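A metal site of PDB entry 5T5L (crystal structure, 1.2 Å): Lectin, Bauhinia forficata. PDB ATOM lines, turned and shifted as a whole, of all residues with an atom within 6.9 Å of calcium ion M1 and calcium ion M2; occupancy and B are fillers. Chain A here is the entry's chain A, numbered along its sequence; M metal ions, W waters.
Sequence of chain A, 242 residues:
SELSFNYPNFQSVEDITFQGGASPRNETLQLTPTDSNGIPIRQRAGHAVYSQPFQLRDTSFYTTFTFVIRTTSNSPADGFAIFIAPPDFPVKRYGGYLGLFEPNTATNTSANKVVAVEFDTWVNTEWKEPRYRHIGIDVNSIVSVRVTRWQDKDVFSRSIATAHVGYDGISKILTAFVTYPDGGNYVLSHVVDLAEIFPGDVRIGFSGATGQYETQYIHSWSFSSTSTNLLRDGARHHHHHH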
ATOM      1  N   ASP A  78      15.738 -27.917   9.104  1.00  0.00           N
ATOM      2  CA  ASP A  78      15.159 -26.695   9.614  1.00  0.00           C
ATOM      3  C   ASP A  78      15.678 -26.230  10.966  1.00  0.00           C
ATOM      4  O   ASP A  78      15.395 -25.076  11.351  1.00  0.00           O
ATOM      5  CB  ASP A  78      13.629 -26.845   9.687  1.00  0.00           C
ATOM      6  CG  ASP A  78      13.008 -26.610   8.338  1.00  0.00           C
ATOM      7  OD1 ASP A  78      12.785 -25.395   8.007  1.00  0.00           O
ATOM      8  OD2 ASP A  78      12.830 -27.564   7.556  1.00  0.00           O
ATOM      9  N   GLY A  95       9.482 -29.728   8.562  1.00  0.00           N
ATOM     10  CA  GLY A  95       9.815 -28.458   8.015  1.00  0.00           C
ATOM     11  C   GLY A  95       9.928 -27.372   9.064  1.00  0.00           C
ATOM     12  O   GLY A  95      10.384 -27.612  10.193  1.00  0.00           O
ATOM     13  N   GLY A  96       9.555 -26.153   8.660  1.00  0.00           N
ATOM     14  CA  GLY A  96       9.814 -24.996   9.516  1.00  0.00           C
ATOM     15  C   GLY A  96       9.006 -24.956  10.783  1.00  0.00           C
ATOM     16  O   GLY A  96       9.270 -24.149  11.675  1.00  0.00           O
ATOM     17  N   TYR A  97       8.015 -25.842  10.905  1.00  0.00           N
ATOM     18  CA  TYR A  97       7.254 -25.981  12.151  1.00  0.00           C
ATOM     19  C   TYR A  97       8.019 -26.681  13.248  1.00  0.00           C
ATOM     20  O   TYR A  97       7.554 -26.707  14.399  1.00  0.00           O
ATOM     21  CB  TYR A  97       5.961 -26.737  11.856  1.00  0.00           C
ATOM     22  CG  TYR A  97       5.135 -26.036  10.779  1.00  0.00           C
ATOM     23  CD1 TYR A  97       4.457 -24.863  11.016  1.00  0.00           C
ATOM     24  CD2 TYR A  97       5.136 -26.528   9.499  1.00  0.00           C
ATOM     25  CE1 TYR A  97       3.795 -24.192  10.006  1.00  0.00           C
ATOM     26  CE2 TYR A  97       4.477 -25.864   8.451  1.00  0.00           C
ATOM     27  CZ  TYR A  97       3.815 -24.700   8.721  1.00  0.00           C
ATOM     28  OH  TYR A  97       3.145 -24.039   7.714  1.00  0.00           O
ATOM     29  N   LEU A  98       9.205 -27.241  12.923  1.00  0.00           N
ATOM     30  CA  LEU A  98      10.135 -27.740  13.907  1.00  0.00           C
ATOM     31  C   LEU A  98       9.621 -28.898  14.724  1.00  0.00           C
ATOM     32  O   LEU A  98      10.137 -29.169  15.825  1.00  0.00           O
ATOM     33  CB  LEU A  98      10.736 -26.630  14.785  1.00  0.00           C
ATOM     34  CG  LEU A  98      11.582 -25.606  14.085  1.00  0.00           C
ATOM     35  CD1 LEU A  98      11.993 -24.496  15.032  1.00  0.00           C
ATOM     36  CD2 LEU A  98      12.809 -26.232  13.467  1.00  0.00           C
ATOM     37  N   GLU A 118      14.457 -22.301  20.295  1.00  0.00           N
ATOM     38  CA  GLU A 118      14.703 -22.841  18.958  1.00  0.00           C
ATOM     39  C   GLU A 118      16.032 -22.397  18.438  1.00  0.00           C
ATOM     40  O   GLU A 118      16.517 -21.281  18.679  1.00  0.00           O
ATOM     41  CB  GLU A 118      13.574 -22.437  17.980  1.00  0.00           C
ATOM     42  CG  GLU A 118      13.481 -20.956  17.698  1.00  0.00           C
ATOM     43  CD  GLU A 118      12.608 -20.666  16.498  1.00  0.00           C
ATOM     44  OE1 GLU A 118      11.448 -21.127  16.468  1.00  0.00           O
ATOM     45  OE2 GLU A 118      13.058 -19.925  15.607  1.00  0.00           O
ATOM     46  N   PHE A 119      16.616 -23.285  17.615  1.00  0.00           N
ATOM     47  CA  PHE A 119      17.855 -23.104  16.880  1.00  0.00           C
ATOM     48  C   PHE A 119      17.483 -23.284  15.421  1.00  0.00           C
ATOM     49  O   PHE A 119      17.282 -24.406  14.952  1.00  0.00           O
ATOM     50  CB  PHE A 119      18.878 -24.167  17.336  1.00  0.00           C
ATOM     51  CG  PHE A 119      19.225 -24.071  18.796  1.00  0.00           C
ATOM     52  CD1 PHE A 119      18.338 -24.593  19.764  1.00  0.00           C
ATOM     53  CD2 PHE A 119      20.411 -23.509  19.221  1.00  0.00           C
ATOM     54  CE1 PHE A 119      18.634 -24.458  21.101  1.00  0.00           C
ATOM     55  CE2 PHE A 119      20.713 -23.409  20.579  1.00  0.00           C
ATOM     56  CZ  PHE A 119      19.826 -23.880  21.509  1.00  0.00           C
ATOM     57  N   ASP A 120      17.282 -22.167  14.729  1.00  0.00           N
ATOM     58  CA  ASP A 120      16.545 -22.153  13.449  1.00  0.00           C
ATOM     59  C   ASP A 120      17.518 -21.904  12.307  1.00  0.00           C
ATOM     60  O   ASP A 120      18.121 -20.829  12.165  1.00  0.00           O
ATOM     61  CB  ASP A 120      15.455 -21.066  13.527  1.00  0.00           C
ATOM     62  CG  ASP A 120      14.536 -21.138  12.400  1.00  0.00           C
ATOM     63  OD1 ASP A 120      14.869 -21.678  11.304  1.00  0.00           O
ATOM     64  OD2 ASP A 120      13.345 -20.636  12.526  1.00  0.00           O
ATOM     65  N   THR A 121      17.709 -22.943  11.458  1.00  0.00           N
ATOM     66  CA  THR A 121      18.679 -22.905  10.377  1.00  0.00           C
ATOM     67  C   THR A 121      18.123 -22.426   9.052  1.00  0.00           C
ATOM     68  O   THR A 121      18.926 -22.281   8.116  1.00  0.00           O
ATOM     69  CB  THR A 121      19.320 -24.294  10.165  1.00  0.00           C
ATOM     70  OG1 THR A 121      18.251 -25.209   9.849  1.00  0.00           O
ATOM     71  CG2 THR A 121      20.072 -24.808  11.393  1.00  0.00           C
ATOM     72  N   TRP A 122      16.810 -22.230   8.931  1.00  0.00           N
ATOM     73  CA  TRP A 122      16.197 -21.931   7.637  1.00  0.00           C
ATOM     74  C   TRP A 122      15.221 -20.770   7.821  1.00  0.00           C
ATOM     75  O   TRP A 122      14.251 -20.829   8.592  1.00  0.00           O
ATOM     76  CB  TRP A 122      15.442 -23.173   7.092  1.00  0.00           C
ATOM     77  CG  TRP A 122      14.722 -22.882   5.823  1.00  0.00           C
ATOM     78  CD1 TRP A 122      13.467 -22.324   5.748  1.00  0.00           C
ATOM     79  CD2 TRP A 122      15.129 -23.107   4.481  1.00  0.00           C
ATOM     80  NE1 TRP A 122      13.091 -22.187   4.430  1.00  0.00           N
ATOM     81  CE2 TRP A 122      14.092 -22.651   3.625  1.00  0.00           C
ATOM     82  CE3 TRP A 122      16.266 -23.622   3.914  1.00  0.00           C
ATOM     83  CZ2 TRP A 122      14.176 -22.732   2.234  1.00  0.00           C
ATOM     84  CZ3 TRP A 122      16.332 -23.753   2.549  1.00  0.00           C
ATOM     85  CH2 TRP A 122      15.293 -23.306   1.713  1.00  0.00           C
ATOM     86  N   VAL A 123      15.472 -19.715   7.074  1.00  0.00           N
ATOM     87  CA  VAL A 123      14.654 -18.514   7.127  1.00  0.00           C
ATOM     88  C   VAL A 123      13.322 -18.766   6.357  1.00  0.00           C
ATOM     89  O   VAL A 123      13.314 -18.877   5.130  1.00  0.00           O
ATOM     90  CB  VAL A 123      15.346 -17.287   6.528  1.00  0.00           C
ATOM     91  CG1 VAL A 123      14.382 -16.074   6.486  1.00  0.00           C
ATOM     92  CG2 VAL A 123      16.557 -16.971   7.403  1.00  0.00           C
ATOM     93  N   ASN A 124      12.210 -18.924   7.096  1.00  0.00           N
ATOM     94  CA  ASN A 124      10.918 -19.167   6.453  1.00  0.00           C
ATOM     95  C   ASN A 124      10.322 -17.873   5.977  1.00  0.00           C
ATOM     96  O   ASN A 124      10.306 -16.894   6.673  1.00  0.00           O
ATOM     97  CB  ASN A 124       9.993 -19.853   7.457  1.00  0.00           C
ATOM     98  CG  ASN A 124      10.354 -21.329   7.600  1.00  0.00           C
ATOM     99  OD1 ASN A 124      11.189 -21.684   8.491  1.00  0.00           O
ATOM    100  ND2 ASN A 124       9.865 -22.158   6.725  1.00  0.00           N
ATOM    101  N   TRP A 127       5.885 -17.195   7.477  1.00  0.00           N
ATOM    102  CA  TRP A 127       5.503 -16.438   8.638  1.00  0.00           C
ATOM    103  C   TRP A 127       6.685 -15.512   8.921  1.00  0.00           C
ATOM    104  O   TRP A 127       7.730 -15.640   8.305  1.00  0.00           O
ATOM    105  CB  TRP A 127       5.212 -17.309   9.875  1.00  0.00           C
ATOM    106  CG  TRP A 127       6.292 -18.310  10.174  1.00  0.00           C
ATOM    107  CD1 TRP A 127       7.464 -18.093  10.892  1.00  0.00           C
ATOM    108  CD2 TRP A 127       6.333 -19.644   9.686  1.00  0.00           C
ATOM    109  NE1 TRP A 127       8.208 -19.275  10.879  1.00  0.00           N
ATOM    110  CE2 TRP A 127       7.529 -20.238  10.141  1.00  0.00           C
ATOM    111  CE3 TRP A 127       5.432 -20.417   8.952  1.00  0.00           C
ATOM    112  CZ2 TRP A 127       7.829 -21.571   9.911  1.00  0.00           C
ATOM    113  CZ3 TRP A 127       5.759 -21.740   8.705  1.00  0.00           C
ATOM    114  CH2 TRP A 127       6.954 -22.297   9.155  1.00  0.00           C
ATOM    115  N   LYS A 128       6.460 -14.596   9.841  1.00  0.00           N
ATOM    116  CA  LYS A 128       7.500 -13.617  10.139  1.00  0.00           C
ATOM    117  C   LYS A 128       8.663 -14.253  10.893  1.00  0.00           C
ATOM    118  O   LYS A 128       8.486 -14.816  11.969  1.00  0.00           O
ATOM    119  CB  LYS A 128       6.915 -12.524  11.068  1.00  0.00           C
ATOM    120  CG  LYS A 128       7.907 -11.446  11.466  1.00  0.00           C
ATOM    121  CD  LYS A 128       7.305 -10.208  12.085  1.00  0.00           C
ATOM    122  CE  LYS A 128       6.866 -10.452  13.522  1.00  0.00           C
ATOM    123  NZ  LYS A 128       7.992 -10.593  14.508  1.00  0.00           N
ATOM    124  N   GLU A 129       9.850 -14.110  10.358  1.00  0.00           N
ATOM    125  CA  GLU A 129      11.054 -14.386  11.122  1.00  0.00           C
ATOM    126  C   GLU A 129      12.237 -13.628  10.526  1.00  0.00           C
ATOM    127  O   GLU A 129      12.076 -12.962   9.504  1.00  0.00           O
ATOM    128  CB  GLU A 129      11.223 -15.891  11.425  1.00  0.00           C
ATOM    129  CG  GLU A 129      11.196 -16.843  10.243  1.00  0.00           C
ATOM    130  CD  GLU A 129      11.597 -18.224  10.679  1.00  0.00           C
ATOM    131  OE1 GLU A 129      11.252 -18.493  11.818  1.00  0.00           O
ATOM    132  OE2 GLU A 129      12.245 -18.966   9.943  1.00  0.00           O
ATOM    133  N   PRO A 130      13.272 -13.422  11.320  1.00  0.00           N
ATOM    134  CA  PRO A 130      14.383 -12.597  10.861  1.00  0.00           C
ATOM    135  C   PRO A 130      14.982 -13.113   9.558  1.00  0.00           C
ATOM    136  O   PRO A 130      14.929 -14.267   9.303  1.00  0.00           O
ATOM    137  CB  PRO A 130      15.375 -12.657  11.996  1.00  0.00           C
ATOM    138  CG  PRO A 130      14.878 -13.541  12.984  1.00  0.00           C
ATOM    139  CD  PRO A 130      13.552 -14.069  12.620  1.00  0.00           C
ATOM    140  N   HIS A 134      18.866 -17.952  13.274  1.00  0.00           N
ATOM    141  CA  HIS A 134      18.577 -17.294  14.535  1.00  0.00           C
ATOM    142  C   HIS A 134      18.292 -18.318  15.620  1.00  0.00           C
ATOM    143  O   HIS A 134      17.897 -19.446  15.339  1.00  0.00           O
ATOM    144  CB  HIS A 134      17.382 -16.310  14.387  1.00  0.00           C
ATOM    145  CG  HIS A 134      16.171 -16.923  13.763  1.00  0.00           C
ATOM    146  ND1 HIS A 134      16.022 -17.058  12.389  1.00  0.00           N
ATOM    147  CD2 HIS A 134      15.036 -17.462  14.293  1.00  0.00           C
ATOM    148  CE1 HIS A 134      14.844 -17.620  12.140  1.00  0.00           C
ATOM    149  NE2 HIS A 134      14.242 -17.892  13.279  1.00  0.00           N
ATOM    150  N   GLY A 136      15.846 -18.439  19.108  1.00  0.00           N
ATOM    151  CA  GLY A 136      14.675 -17.734  19.610  1.00  0.00           C
ATOM    152  C   GLY A 136      13.996 -18.417  20.753  1.00  0.00           C
ATOM    153  O   GLY A 136      14.172 -19.606  20.985  1.00  0.00           O
ATOM    154  N   ASP A 138      10.210 -19.226  21.891  1.00  0.00           N
ATOM    155  CA  ASP A 138       8.869 -19.365  21.336  1.00  0.00           C
ATOM    156  C   ASP A 138       7.900 -19.642  22.462  1.00  0.00           C
ATOM    157  O   ASP A 138       8.125 -20.500  23.300  1.00  0.00           O
ATOM    158  CB  ASP A 138       8.834 -20.564  20.350  1.00  0.00           C
ATOM    159  CG  ASP A 138       9.755 -20.425  19.186  1.00  0.00           C
ATOM    160  OD1 ASP A 138      10.231 -19.324  18.880  1.00  0.00           O
ATOM    161  OD2 ASP A 138      10.020 -21.515  18.546  1.00  0.00           O
ATOM    162  N   ILE A 142       5.159 -20.261  16.388  1.00  0.00           N
ATOM    163  CA  ILE A 142       6.429 -20.400  15.650  1.00  0.00           C
ATOM    164  C   ILE A 142       7.083 -19.045  15.360  1.00  0.00           C
ATOM    165  O   ILE A 142       8.241 -18.992  14.970  1.00  0.00           O
ATOM    166  CB  ILE A 142       6.193 -21.220  14.334  1.00  0.00           C
ATOM    167  CG1 ILE A 142       7.466 -21.822  13.728  1.00  0.00           C
ATOM    168  CG2 ILE A 142       5.405 -20.422  13.292  1.00  0.00           C
ATOM    169  CD1 ILE A 142       8.306 -22.747  14.630  1.00  0.00           C
ATOM    170  N   VAL A 143       6.353 -17.952  15.582  1.00  0.00           N
ATOM    171  CA  VAL A 143       6.910 -16.599  15.471  1.00  0.00           C
ATOM    172  C   VAL A 143       7.484 -16.249  16.834  1.00  0.00           C
ATOM    173  O   VAL A 143       6.737 -15.990  17.799  1.00  0.00           O
ATOM    174  CB  VAL A 143       5.870 -15.573  15.008  1.00  0.00           C
ATOM    175  CG1 VAL A 143       6.485 -14.174  15.007  1.00  0.00           C
ATOM    176  CG2 VAL A 143       5.385 -15.914  13.584  1.00  0.00           C
ATOM    177  N   SER A 144       8.798 -16.279  16.968  1.00  0.00           N
ATOM    178  CA  SER A 144       9.450 -16.128  18.277  1.00  0.00           C
ATOM    179  C   SER A 144       9.106 -14.787  18.932  1.00  0.00           C
ATOM    180  O   SER A 144       9.032 -13.751  18.295  1.00  0.00           O
ATOM    181  CB  SER A 144      10.956 -16.215  18.086  1.00  0.00           C
ATOM    182  OG  SER A 144      11.400 -17.391  17.473  1.00  0.00           O
ATOM    183  N   VAL A 147      14.222 -13.034  19.706  1.00  0.00           N
ATOM    184  CA  VAL A 147      15.019 -13.697  18.708  1.00  0.00           C
ATOM    185  C   VAL A 147      16.296 -12.958  18.464  1.00  0.00           C
ATOM    186  O   VAL A 147      16.276 -11.671  18.430  1.00  0.00           O
ATOM    187  CB  VAL A 147      14.134 -13.918  17.424  1.00  0.00           C
ATOM    188  CG1 VAL A 147      13.805 -12.570  16.699  1.00  0.00           C
ATOM    189  CG2 VAL A 147      14.727 -14.917  16.485  1.00  0.00           C
HETATM  190 CA    CA M   1      12.685 -21.299  10.243  1.00  0.00          CA
HETATM  191 CA    CA M   2      12.349 -19.117  13.666  1.00  0.00          CA
HETATM  192  O   HOH W   1      11.648 -17.400  14.779  1.00  0.00           O
HETATM  193  O   HOH W   2      13.191 -23.618  10.028  1.00  0.00           O
HETATM  194  O   HOH W   3      10.548 -20.359  14.099  1.00  0.00           O
HETATM  195  O   HOH W   4      10.838 -21.876  11.659  1.00  0.00           O
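Water W3 bridges the side-chain carboxylate of Glu 118 (2.6 Å) and the backbone carbonyl oxygen of Ile 142 (2.8 Å).
Of the 23 residues printed, 4 come within 4 Å of calcium ion M1.
The nearest printed residue that does not touch calcium ion M1 is Val 123 (4.5 Å).
Calcium ion M1 is bound by O of Trp 122 (2.3 Å).
OD1 of Asn 124 binds calcium ion M1.
Calcium ion M1 is bound by water W2, at 2.4 Å.
Calcium ion M1 is bound by OE2 of Glu 129 (2.4 Å).
Water W4 binds calcium ion M1 (2.4 Å).
Calcium ion M1 is bound by OD1 of Asp 120, at 2.5 Å.
The side-chain carboxylate (OD2) of Asp 120 is bound to calcium ion M1, at 2.5 Å.
The side-chain carboxylate (OD2) of Asp 138 lies close to the side-chain carboxylate (OE1) of Glu 118 (2.6 Å).
N of Glu 118 sits at hydrogen-bond distance from O of Gly 136, 2.8 Å away.
NE1 of Trp 127 lies close to OE1 of Glu 129 (3.3 Å).
Calcium ion M2 is bound by OD2 of Asp 120 (2.1 Å), water W1 (2.2 Å), OE2 of Glu 118 (2.2 Å), water W3 (2.2 Å), OE1 of Glu 129 (2.2 Å) and NE2 of His 134 (2.3 Å).
Calcium ion M2 has six donor atoms within binding distance.
Of the 23 residues printed, 4 come within 4 Å of calcium ion M2.
The nearest printed residue that does not touch calcium ion M2 is Ser 144 (4.3 Å).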
